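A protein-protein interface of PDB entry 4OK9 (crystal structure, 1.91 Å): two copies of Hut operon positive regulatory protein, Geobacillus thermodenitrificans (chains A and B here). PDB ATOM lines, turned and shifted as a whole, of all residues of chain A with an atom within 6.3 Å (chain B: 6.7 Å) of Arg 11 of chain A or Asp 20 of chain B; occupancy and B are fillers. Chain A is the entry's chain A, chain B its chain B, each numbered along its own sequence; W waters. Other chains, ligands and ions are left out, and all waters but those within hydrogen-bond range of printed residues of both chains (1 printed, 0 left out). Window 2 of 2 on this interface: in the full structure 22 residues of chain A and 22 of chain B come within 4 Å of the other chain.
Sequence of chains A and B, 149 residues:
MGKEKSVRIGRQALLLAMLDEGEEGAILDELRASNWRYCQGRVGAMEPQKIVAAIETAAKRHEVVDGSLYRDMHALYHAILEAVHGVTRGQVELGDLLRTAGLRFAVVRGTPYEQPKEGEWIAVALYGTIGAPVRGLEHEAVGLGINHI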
ATOM      1  N   ARG A   8      -3.890  23.388  -5.277  1.00  0.00           N
ATOM      2  CA  ARG A   8      -3.556  22.366  -6.302  1.00  0.00           C
ATOM      3  C   ARG A   8      -3.548  23.007  -7.690  1.00  0.00           C
ATOM      4  O   ARG A   8      -4.476  22.865  -8.513  1.00  0.00           O
ATOM      5  CB  ARG A   8      -4.473  21.120  -6.210  1.00  0.00           C
ATOM      6  CG  ARG A   8      -4.297  20.299  -4.950  1.00  0.00           C
ATOM      7  CD  ARG A   8      -2.878  19.900  -4.684  1.00  0.00           C
ATOM      8  NE  ARG A   8      -2.713  18.824  -3.670  1.00  0.00           N
ATOM      9  CZ  ARG A   8      -2.828  17.499  -3.866  1.00  0.00           C
ATOM     10  NH1 ARG A   8      -3.190  16.970  -5.019  1.00  0.00           N
ATOM     11  NH2 ARG A   8      -2.634  16.687  -2.849  1.00  0.00           N
ATOM     12  N   ILE A   9      -2.462  23.765  -7.918  1.00  0.00           N
ATOM     13  CA  ILE A   9      -2.234  24.482  -9.153  1.00  0.00           C
ATOM     14  C   ILE A   9      -2.245  23.626 -10.429  1.00  0.00           C
ATOM     15  O   ILE A   9      -2.842  24.026 -11.432  1.00  0.00           O
ATOM     16  CB  ILE A   9      -0.914  25.308  -9.046  1.00  0.00           C
ATOM     17  CG1 ILE A   9      -0.827  26.285 -10.202  1.00  0.00           C
ATOM     18  CG2 ILE A   9       0.352  24.438  -8.891  1.00  0.00           C
ATOM     19  CD1 ILE A   9       0.284  27.267 -10.028  1.00  0.00           C
ATOM     20  N   GLY A  10      -1.699  22.443 -10.324  1.00  0.00           N
ATOM     21  CA  GLY A  10      -1.746  21.467 -11.409  1.00  0.00           C
ATOM     22  C   GLY A  10      -3.152  21.036 -11.683  1.00  0.00           C
ATOM     23  O   GLY A  10      -3.569  20.952 -12.771  1.00  0.00           O
ATOM     24  N   ARG A  11      -3.904  20.745 -10.626  1.00  0.00           N
ATOM     25  CA  ARG A  11      -5.286  20.347 -10.836  1.00  0.00           C
ATOM     26  C   ARG A  11      -6.066  21.482 -11.378  1.00  0.00           C
ATOM     27  O   ARG A  11      -6.912  21.255 -12.255  1.00  0.00           O
ATOM     28  CB  ARG A  11      -5.934  19.826  -9.509  1.00  0.00           C
ATOM     29  CG  ARG A  11      -7.417  19.557  -9.716  1.00  0.00           C
ATOM     30  CD  ARG A  11      -8.155  19.034  -8.499  1.00  0.00           C
ATOM     31  NE  ARG A  11      -7.902  19.852  -7.354  1.00  0.00           N
ATOM     32  CZ  ARG A  11      -8.364  19.586  -6.148  1.00  0.00           C
ATOM     33  NH1 ARG A  11      -9.174  18.533  -5.952  1.00  0.00           N
ATOM     34  NH2 ARG A  11      -8.027  20.383  -5.144  1.00  0.00           N
ATOM     35  N   GLN A  12      -5.793  22.724 -10.941  1.00  0.00           N
ATOM     36  CA  GLN A  12      -6.427  23.852 -11.674  1.00  0.00           C
ATOM     37  C   GLN A  12      -6.146  23.872 -13.123  1.00  0.00           C
ATOM     38  O   GLN A  12      -7.067  23.966 -13.946  1.00  0.00           O
ATOM     39  CB  GLN A  12      -6.050  25.214 -11.125  1.00  0.00           C
ATOM     40  CG  GLN A  12      -6.508  25.461  -9.675  1.00  0.00           C
ATOM     41  CD  GLN A  12      -5.930  26.727  -9.093  1.00  0.00           C
ATOM     42  OE1 GLN A  12      -4.775  27.093  -9.363  1.00  0.00           O
ATOM     43  NE2 GLN A  12      -6.747  27.444  -8.294  1.00  0.00           N
ATOM     44  N   ALA A  13      -4.868  23.755 -13.517  1.00  0.00           N
ATOM     45  CA  ALA A  13      -4.564  23.732 -14.986  1.00  0.00           C
ATOM     46  C   ALA A  13      -5.277  22.634 -15.818  1.00  0.00           C
ATOM     47  O   ALA A  13      -5.815  22.824 -16.909  1.00  0.00           O
ATOM     48  CB  ALA A  13      -3.035  23.730 -15.196  1.00  0.00           C
ATOM     49  N   LEU A  14      -5.323  21.443 -15.237  1.00  0.00           N
ATOM     50  CA  LEU A  14      -5.967  20.316 -15.813  1.00  0.00           C
ATOM     51  C   LEU A  14      -7.425  20.515 -15.961  1.00  0.00           C
ATOM     52  O   LEU A  14      -7.979  20.243 -16.992  1.00  0.00           O
ATOM     53  CB  LEU A  14      -5.714  19.125 -14.875  1.00  0.00           C
ATOM     54  CG  LEU A  14      -4.300  18.512 -14.909  1.00  0.00           C
ATOM     55  CD1 LEU A  14      -4.052  17.511 -13.796  1.00  0.00           C
ATOM     56  CD2 LEU A  14      -4.136  17.798 -16.249  1.00  0.00           C
ATOM     57  N   LEU A  15      -8.050  21.055 -14.943  1.00  0.00           N
ATOM     58  CA  LEU A  15      -9.480  21.351 -15.076  1.00  0.00           C
ATOM     59  C   LEU A  15      -9.788  22.345 -16.171  1.00  0.00           C
ATOM     60  O   LEU A  15     -10.743  22.184 -16.944  1.00  0.00           O
ATOM     61  CB  LEU A  15      -9.961  21.796 -13.672  1.00  0.00           C
ATOM     62  CG  LEU A  15     -10.136  20.638 -12.685  1.00  0.00           C
ATOM     63  CD1 LEU A  15     -10.564  21.131 -11.300  1.00  0.00           C
ATOM     64  CD2 LEU A  15     -11.135  19.581 -13.157  1.00  0.00           C
ATOM     65  N   LEU A  16      -8.947  23.363 -16.299  1.00  0.00           N
ATOM     66  CA  LEU A  16      -9.111  24.277 -17.407  1.00  0.00           C
ATOM     67  C   LEU A  16      -8.902  23.593 -18.701  1.00  0.00           C
ATOM     68  O   LEU A  16      -9.612  23.898 -19.666  1.00  0.00           O
ATOM     69  CB  LEU A  16      -8.142  25.476 -17.362  1.00  0.00           C
ATOM     70  CG  LEU A  16      -8.187  26.404 -16.179  1.00  0.00           C
ATOM     71  CD1 LEU A  16      -7.169  27.494 -16.438  1.00  0.00           C
ATOM     72  CD2 LEU A  16      -9.605  26.950 -15.992  1.00  0.00           C
ATOM     73  N   MET A  18      -9.517  20.316 -19.316  1.00  0.00           N
ATOM     74  CA  MET A  18     -10.458  19.238 -19.640  1.00  0.00           C
ATOM     75  C   MET A  18     -11.940  19.553 -19.500  1.00  0.00           C
ATOM     76  O   MET A  18     -12.710  19.006 -20.244  1.00  0.00           O
ATOM     77  CB  MET A  18     -10.079  17.929 -18.950  1.00  0.00           C
ATOM     78  CG  MET A  18     -10.379  17.798 -17.496  1.00  0.00           C
ATOM     79  SD  MET A  18      -9.702  16.269 -16.732  1.00  0.00           S
ATOM     80  CE  MET A  18      -8.075  16.867 -16.549  1.00  0.00           C
ATOM     81  N   ILE A  27     -13.164  27.656 -11.391  1.00  0.00           N
ATOM     82  CA  ILE A  27     -11.704  27.708 -11.512  1.00  0.00           C
ATOM     83  C   ILE A  27     -11.280  29.118 -11.920  1.00  0.00           C
ATOM     84  O   ILE A  27     -10.399  29.689 -11.319  1.00  0.00           O
ATOM     85  CB  ILE A  27     -11.104  26.671 -12.527  1.00  0.00           C
ATOM     86  CG1 ILE A  27     -11.750  25.289 -12.351  1.00  0.00           C
ATOM     87  CG2 ILE A  27      -9.585  26.591 -12.346  1.00  0.00           C
ATOM     88  CD1 ILE A  27     -11.516  24.744 -10.972  1.00  0.00           C
ATOM     89  N   LEU A 144       0.684  16.616 -17.418  1.00  0.00           N
ATOM     90  CA  LEU A 144       0.909  17.720 -16.537  1.00  0.00           C
ATOM     91  C   LEU A 144       2.386  17.893 -16.258  1.00  0.00           C
ATOM     92  O   LEU A 144       3.052  16.970 -15.926  1.00  0.00           O
ATOM     93  CB  LEU A 144       0.192  17.508 -15.227  1.00  0.00           C
ATOM     94  CG  LEU A 144       0.431  18.568 -14.180  1.00  0.00           C
ATOM     95  CD1 LEU A 144      -0.143  19.886 -14.622  1.00  0.00           C
ATOM     96  CD2 LEU A 144      -0.110  18.168 -12.840  1.00  0.00           C
ATOM     97  N   LEU B  15     -11.366  12.802 -13.772  1.00  0.00           N
ATOM     98  CA  LEU B  15     -12.216  13.488 -12.787  1.00  0.00           C
ATOM     99  C   LEU B  15     -12.446  12.691 -11.471  1.00  0.00           C
ATOM    100  O   LEU B  15     -12.346  13.250 -10.379  1.00  0.00           O
ATOM    101  CB  LEU B  15     -13.505  13.930 -13.470  1.00  0.00           C
ATOM    102  CG  LEU B  15     -13.290  15.109 -14.439  1.00  0.00           C
ATOM    103  CD1 LEU B  15     -14.541  15.525 -15.237  1.00  0.00           C
ATOM    104  CD2 LEU B  15     -12.680  16.290 -13.668  1.00  0.00           C
ATOM    105  N   LEU B  16     -12.617  11.376 -11.554  1.00  0.00           N
ATOM    106  CA  LEU B  16     -12.703  10.581 -10.351  1.00  0.00           C
ATOM    107  C   LEU B  16     -11.456  10.635  -9.537  1.00  0.00           C
ATOM    108  O   LEU B  16     -11.508  10.761  -8.299  1.00  0.00           O
ATOM    109  CB  LEU B  16     -13.076   9.115 -10.637  1.00  0.00           C
ATOM    110  CG  LEU B  16     -14.455   8.781 -11.168  1.00  0.00           C
ATOM    111  CD1 LEU B  16     -14.498   7.266 -11.434  1.00  0.00           C
ATOM    112  CD2 LEU B  16     -15.517   9.194 -10.126  1.00  0.00           C
ATOM    113  N   ALA B  17     -10.319  10.525 -10.195  1.00  0.00           N
ATOM    114  CA  ALA B  17      -9.033  10.576  -9.542  1.00  0.00           C
ATOM    115  C   ALA B  17      -8.696  11.904  -8.928  1.00  0.00           C
ATOM    116  O   ALA B  17      -8.042  11.959  -7.948  1.00  0.00           O
ATOM    117  CB  ALA B  17      -7.941  10.143 -10.478  1.00  0.00           C
ATOM    118  N   MET B  18      -9.081  12.981  -9.576  1.00  0.00           N
ATOM    119  CA  MET B  18      -8.735  14.311  -9.077  1.00  0.00           C
ATOM    120  C   MET B  18      -9.743  15.142  -8.260  1.00  0.00           C
ATOM    121  O   MET B  18      -9.346  15.907  -7.455  1.00  0.00           O
ATOM    122  CB  MET B  18      -8.050  15.137 -10.154  1.00  0.00           C
ATOM    123  CG  MET B  18      -8.920  15.649 -11.251  1.00  0.00           C
ATOM    124  SD  MET B  18      -7.901  16.385 -12.533  1.00  0.00           S
ATOM    125  CE  MET B  18      -7.999  15.160 -13.756  1.00  0.00           C
ATOM    126  N   LEU B  19     -11.028  15.001  -8.493  1.00  0.00           N
ATOM    127  CA  LEU B  19     -12.018  15.752  -7.733  1.00  0.00           C
ATOM    128  C   LEU B  19     -12.091  15.310  -6.303  1.00  0.00           C
ATOM    129  O   LEU B  19     -12.012  14.154  -6.027  1.00  0.00           O
ATOM    130  CB  LEU B  19     -13.380  15.579  -8.343  1.00  0.00           C
ATOM    131  CG  LEU B  19     -13.563  16.133  -9.713  1.00  0.00           C
ATOM    132  CD1 LEU B  19     -14.920  15.826 -10.294  1.00  0.00           C
ATOM    133  CD2 LEU B  19     -13.219  17.593  -9.732  1.00  0.00           C
ATOM    134  N   ASP B  20     -12.274  16.236  -5.385  1.00  0.00           N
ATOM    135  CA  ASP B  20     -12.325  15.887  -3.977  1.00  0.00           C
ATOM    136  C   ASP B  20     -13.514  15.012  -3.715  1.00  0.00           C
ATOM    137  O   ASP B  20     -14.517  15.098  -4.388  1.00  0.00           O
ATOM    138  CB  ASP B  20     -12.471  17.118  -3.103  1.00  0.00           C
ATOM    139  CG  ASP B  20     -11.320  18.060  -3.223  1.00  0.00           C
ATOM    140  OD1 ASP B  20     -10.178  17.630  -3.017  1.00  0.00           O
ATOM    141  OD2 ASP B  20     -11.578  19.221  -3.503  1.00  0.00           O
ATOM    142  N   GLU B  21     -13.397  14.162  -2.720  1.00  0.00           N
ATOM    143  CA  GLU B  21     -14.496  13.297  -2.372  1.00  0.00           C
ATOM    144  C   GLU B  21     -15.673  14.171  -2.011  1.00  0.00           C
ATOM    145  O   GLU B  21     -15.582  15.050  -1.185  1.00  0.00           O
ATOM    146  CB  GLU B  21     -14.082  12.395  -1.214  1.00  0.00           C
ATOM    147  CG  GLU B  21     -12.800  11.621  -1.506  1.00  0.00           C
ATOM    148  CD  GLU B  21     -12.666  10.311  -0.750  1.00  0.00           C
ATOM    149  OE1 GLU B  21     -11.609   9.672  -0.870  1.00  0.00           O
ATOM    150  OE2 GLU B  21     -13.601   9.919  -0.031  1.00  0.00           O
ATOM    151  N   GLY B  22     -16.799  13.852  -2.616  1.00  0.00           N
ATOM    152  CA  GLY B  22     -17.993  14.658  -2.585  1.00  0.00           C
ATOM    153  C   GLY B  22     -18.226  15.635  -3.717  1.00  0.00           C
ATOM    154  O   GLY B  22     -19.286  16.239  -3.796  1.00  0.00           O
ATOM    155  N   GLU B  23     -17.253  15.804  -4.595  1.00  0.00           N
ATOM    156  CA  GLU B  23     -17.455  16.650  -5.738  1.00  0.00           C
ATOM    157  C   GLU B  23     -17.730  15.834  -6.978  1.00  0.00           C
ATOM    158  O   GLU B  23     -18.010  16.382  -8.008  1.00  0.00           O
ATOM    159  CB  GLU B  23     -16.250  17.560  -5.947  1.00  0.00           C
ATOM    160  CG  GLU B  23     -16.473  19.000  -5.526  1.00  0.00           C
ATOM    161  CD  GLU B  23     -15.498  19.994  -6.140  1.00  0.00           C
ATOM    162  OE1 GLU B  23     -14.945  20.800  -5.387  1.00  0.00           O
ATOM    163  OE2 GLU B  23     -15.292  19.993  -7.369  1.00  0.00           O
ATOM    164  N   GLU B  24     -17.662  14.518  -6.867  1.00  0.00           N
ATOM    165  CA  GLU B  24     -17.687  13.658  -8.049  1.00  0.00           C
ATOM    166  C   GLU B  24     -19.027  13.028  -8.439  1.00  0.00           C
ATOM    167  O   GLU B  24     -19.088  12.175  -9.272  1.00  0.00           O
ATOM    168  CB  GLU B  24     -16.591  12.606  -7.981  1.00  0.00           C
ATOM    169  CG  GLU B  24     -16.955  11.368  -7.199  1.00  0.00           C
ATOM    170  CD  GLU B  24     -17.010  11.633  -5.735  1.00  0.00           C
ATOM    171  OE1 GLU B  24     -17.323  12.769  -5.383  1.00  0.00           O
ATOM    172  OE2 GLU B  24     -16.738  10.721  -4.949  1.00  0.00           O
ATOM    173  N   ARG B 104      -3.933   9.049  -6.148  1.00  0.00           N
ATOM    174  CA  ARG B 104      -5.223   8.511  -6.426  1.00  0.00           C
ATOM    175  C   ARG B 104      -5.349   7.935  -7.795  1.00  0.00           C
ATOM    176  O   ARG B 104      -4.783   8.414  -8.795  1.00  0.00           O
ATOM    177  CB  ARG B 104      -6.303   9.562  -6.196  1.00  0.00           C
ATOM    178  CG  ARG B 104      -6.379   9.994  -4.754  1.00  0.00           C
ATOM    179  CD  ARG B 104      -7.402  11.094  -4.540  1.00  0.00           C
ATOM    180  NE  ARG B 104      -8.761  10.630  -4.854  1.00  0.00           N
ATOM    181  CZ  ARG B 104      -9.808  11.428  -5.096  1.00  0.00           C
ATOM    182  NH1 ARG B 104      -9.681  12.762  -5.036  1.00  0.00           N
ATOM    183  NH2 ARG B 104     -11.005  10.887  -5.374  1.00  0.00           N
ATOM    184  N   TYR B 127      -3.817  10.645 -10.326  1.00  0.00           N
ATOM    185  CA  TYR B 127      -3.585  12.053 -10.037  1.00  0.00           C
ATOM    186  C   TYR B 127      -2.986  12.064  -8.635  1.00  0.00           C
ATOM    187  O   TYR B 127      -3.521  11.469  -7.783  1.00  0.00           O
ATOM    188  CB  TYR B 127      -4.803  12.927 -10.137  1.00  0.00           C
ATOM    189  CG  TYR B 127      -4.598  14.255  -9.458  1.00  0.00           C
ATOM    190  CD1 TYR B 127      -3.865  15.252 -10.050  1.00  0.00           C
ATOM    191  CD2 TYR B 127      -5.047  14.460  -8.194  1.00  0.00           C
ATOM    192  CE1 TYR B 127      -3.650  16.437  -9.423  1.00  0.00           C
ATOM    193  CE2 TYR B 127      -4.839  15.646  -7.554  1.00  0.00           C
ATOM    194  CZ  TYR B 127      -4.141  16.637  -8.181  1.00  0.00           C
ATOM    195  OH  TYR B 127      -3.911  17.801  -7.560  1.00  0.00           O
ATOM    196  N   GLU B 140       2.551  18.132  -7.924  1.00  0.00           N
ATOM    197  CA  GLU B 140       1.516  17.348  -8.521  1.00  0.00           C
ATOM    198  C   GLU B 140       2.036  16.570  -9.723  1.00  0.00           C
ATOM    199  O   GLU B 140       3.085  16.908 -10.287  1.00  0.00           O
ATOM    200  CB  GLU B 140       0.370  18.222  -8.927  1.00  0.00           C
ATOM    201  CG  GLU B 140      -0.397  18.757  -7.701  1.00  0.00           C
ATOM    202  CD  GLU B 140      -1.242  19.929  -8.055  1.00  0.00           C
ATOM    203  OE1 GLU B 140      -2.438  19.723  -8.432  1.00  0.00           O
ATOM    204  OE2 GLU B 140      -0.636  21.057  -8.093  1.00  0.00           O
HETATM  205  O   HOH W   1       4.424  16.881 -12.716  1.00  0.00           O
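NH1 of Arg 8 of chain A lies within hydrogen-bond range of OH of Tyr 127 of chain B.
The side-chain carboxylate of Glu 140 of chain B sits at hydrogen-bond distance from the backbone NH of Ile 9 of chain A, 3.3 Å away.
The side-chain carboxylate (OE2) of Glu 140 of chain B sits at hydrogen-bond distance from the backbone NH (N) of Gly 10 of chain A (2.8 Å).
NH1 of Arg 11 of chain A lies within hydrogen-bond range of O of Met 18 of chain B, at 3.0 Å.
The side-chain carboxylate of Asp 20 of chain B lies within salt-bridge range of the guanidinium group of Arg 11 of chain A (3.2 Å).
N of Arg 11 of chain A sits at hydrogen-bond distance from OE1 of Glu 140 of chain B, at 2.8 Å.
O of Arg 104 of chain B is in hydrogen-bond range of N of Tyr 127 of chain B (2.9 Å).
The side-chain hydroxyl (OH) of Tyr 127 of chain B lies within hydrogen-bond range of the side-chain carboxylate (OE1) of Glu 140 of chain B (2.6 Å).
Among the printed residues, pairs that only touch across the chains: Arg 8 of chain A with Glu 140 of chain B, Arg 11 of chain A with Tyr 127 of chain B, Leu 15 of chain A with Leu 15 of chain B, Met 18 of chain A with Met 18 of chain B and Leu 144 of chain A with Glu 140 of chain B.
Of the printed residues of chain B, Arg 8 of chain A touches Tyr 127 (2.8 Å) and Glu 140 (3.3 Å).
Arg 11 of chain A touches just these residues of chain B: Met 18 (3.0 Å), Asp 20 (3.2 Å), Tyr 127 (3.5 Å) and Glu 140 (2.8 Å).
Leu 16 of chain A touches none of the printed residues of chain B.
Of the printed residues of chain B, Leu 144 of chain A touches Glu 140.
Of the printed residues of chain A, Leu 15 of chain B touches Leu 15.
Leu 16 of chain B touches none of the printed residues of chain A.
Asp 20 of chain B touches just one residue of chain A: Arg 11 (3.2 Å).
Of the 13 printed residues of chain B, 5 touch a printed residue of chain A.
Hydrophobic or aromatic side chains of chain B within 4 Å of the printed part of chain A: Leu 15, Met 18 and Tyr 127.
Printed residues of chain A that touch a printed residue of chain B: Arg 8, Ile 9, Gly 10, Arg 11, Leu 15, Met 18 and Leu 144.
Hydrophobic or aromatic side chains of chain A within 4 Å of the printed part of chain B: Ile 9, Leu 15, Met 18 and Leu 144.
Among the printed residues, 11 pairs touch across the chains.
Leu 15 of chain A touches its own counterpart, Leu 15 of chain B.
Met 18 of chain A touches its own counterpart, Met 18 of chain B.
Positions printed for both chains: 15, 16 and 18.
Of the 11 pairs that touch across the chains among the printed residues, 2 have their exchanged pair printed and touching as well.
Water W1 bridges O of Glu 140 of chain B and O of Leu 144 of chain A.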
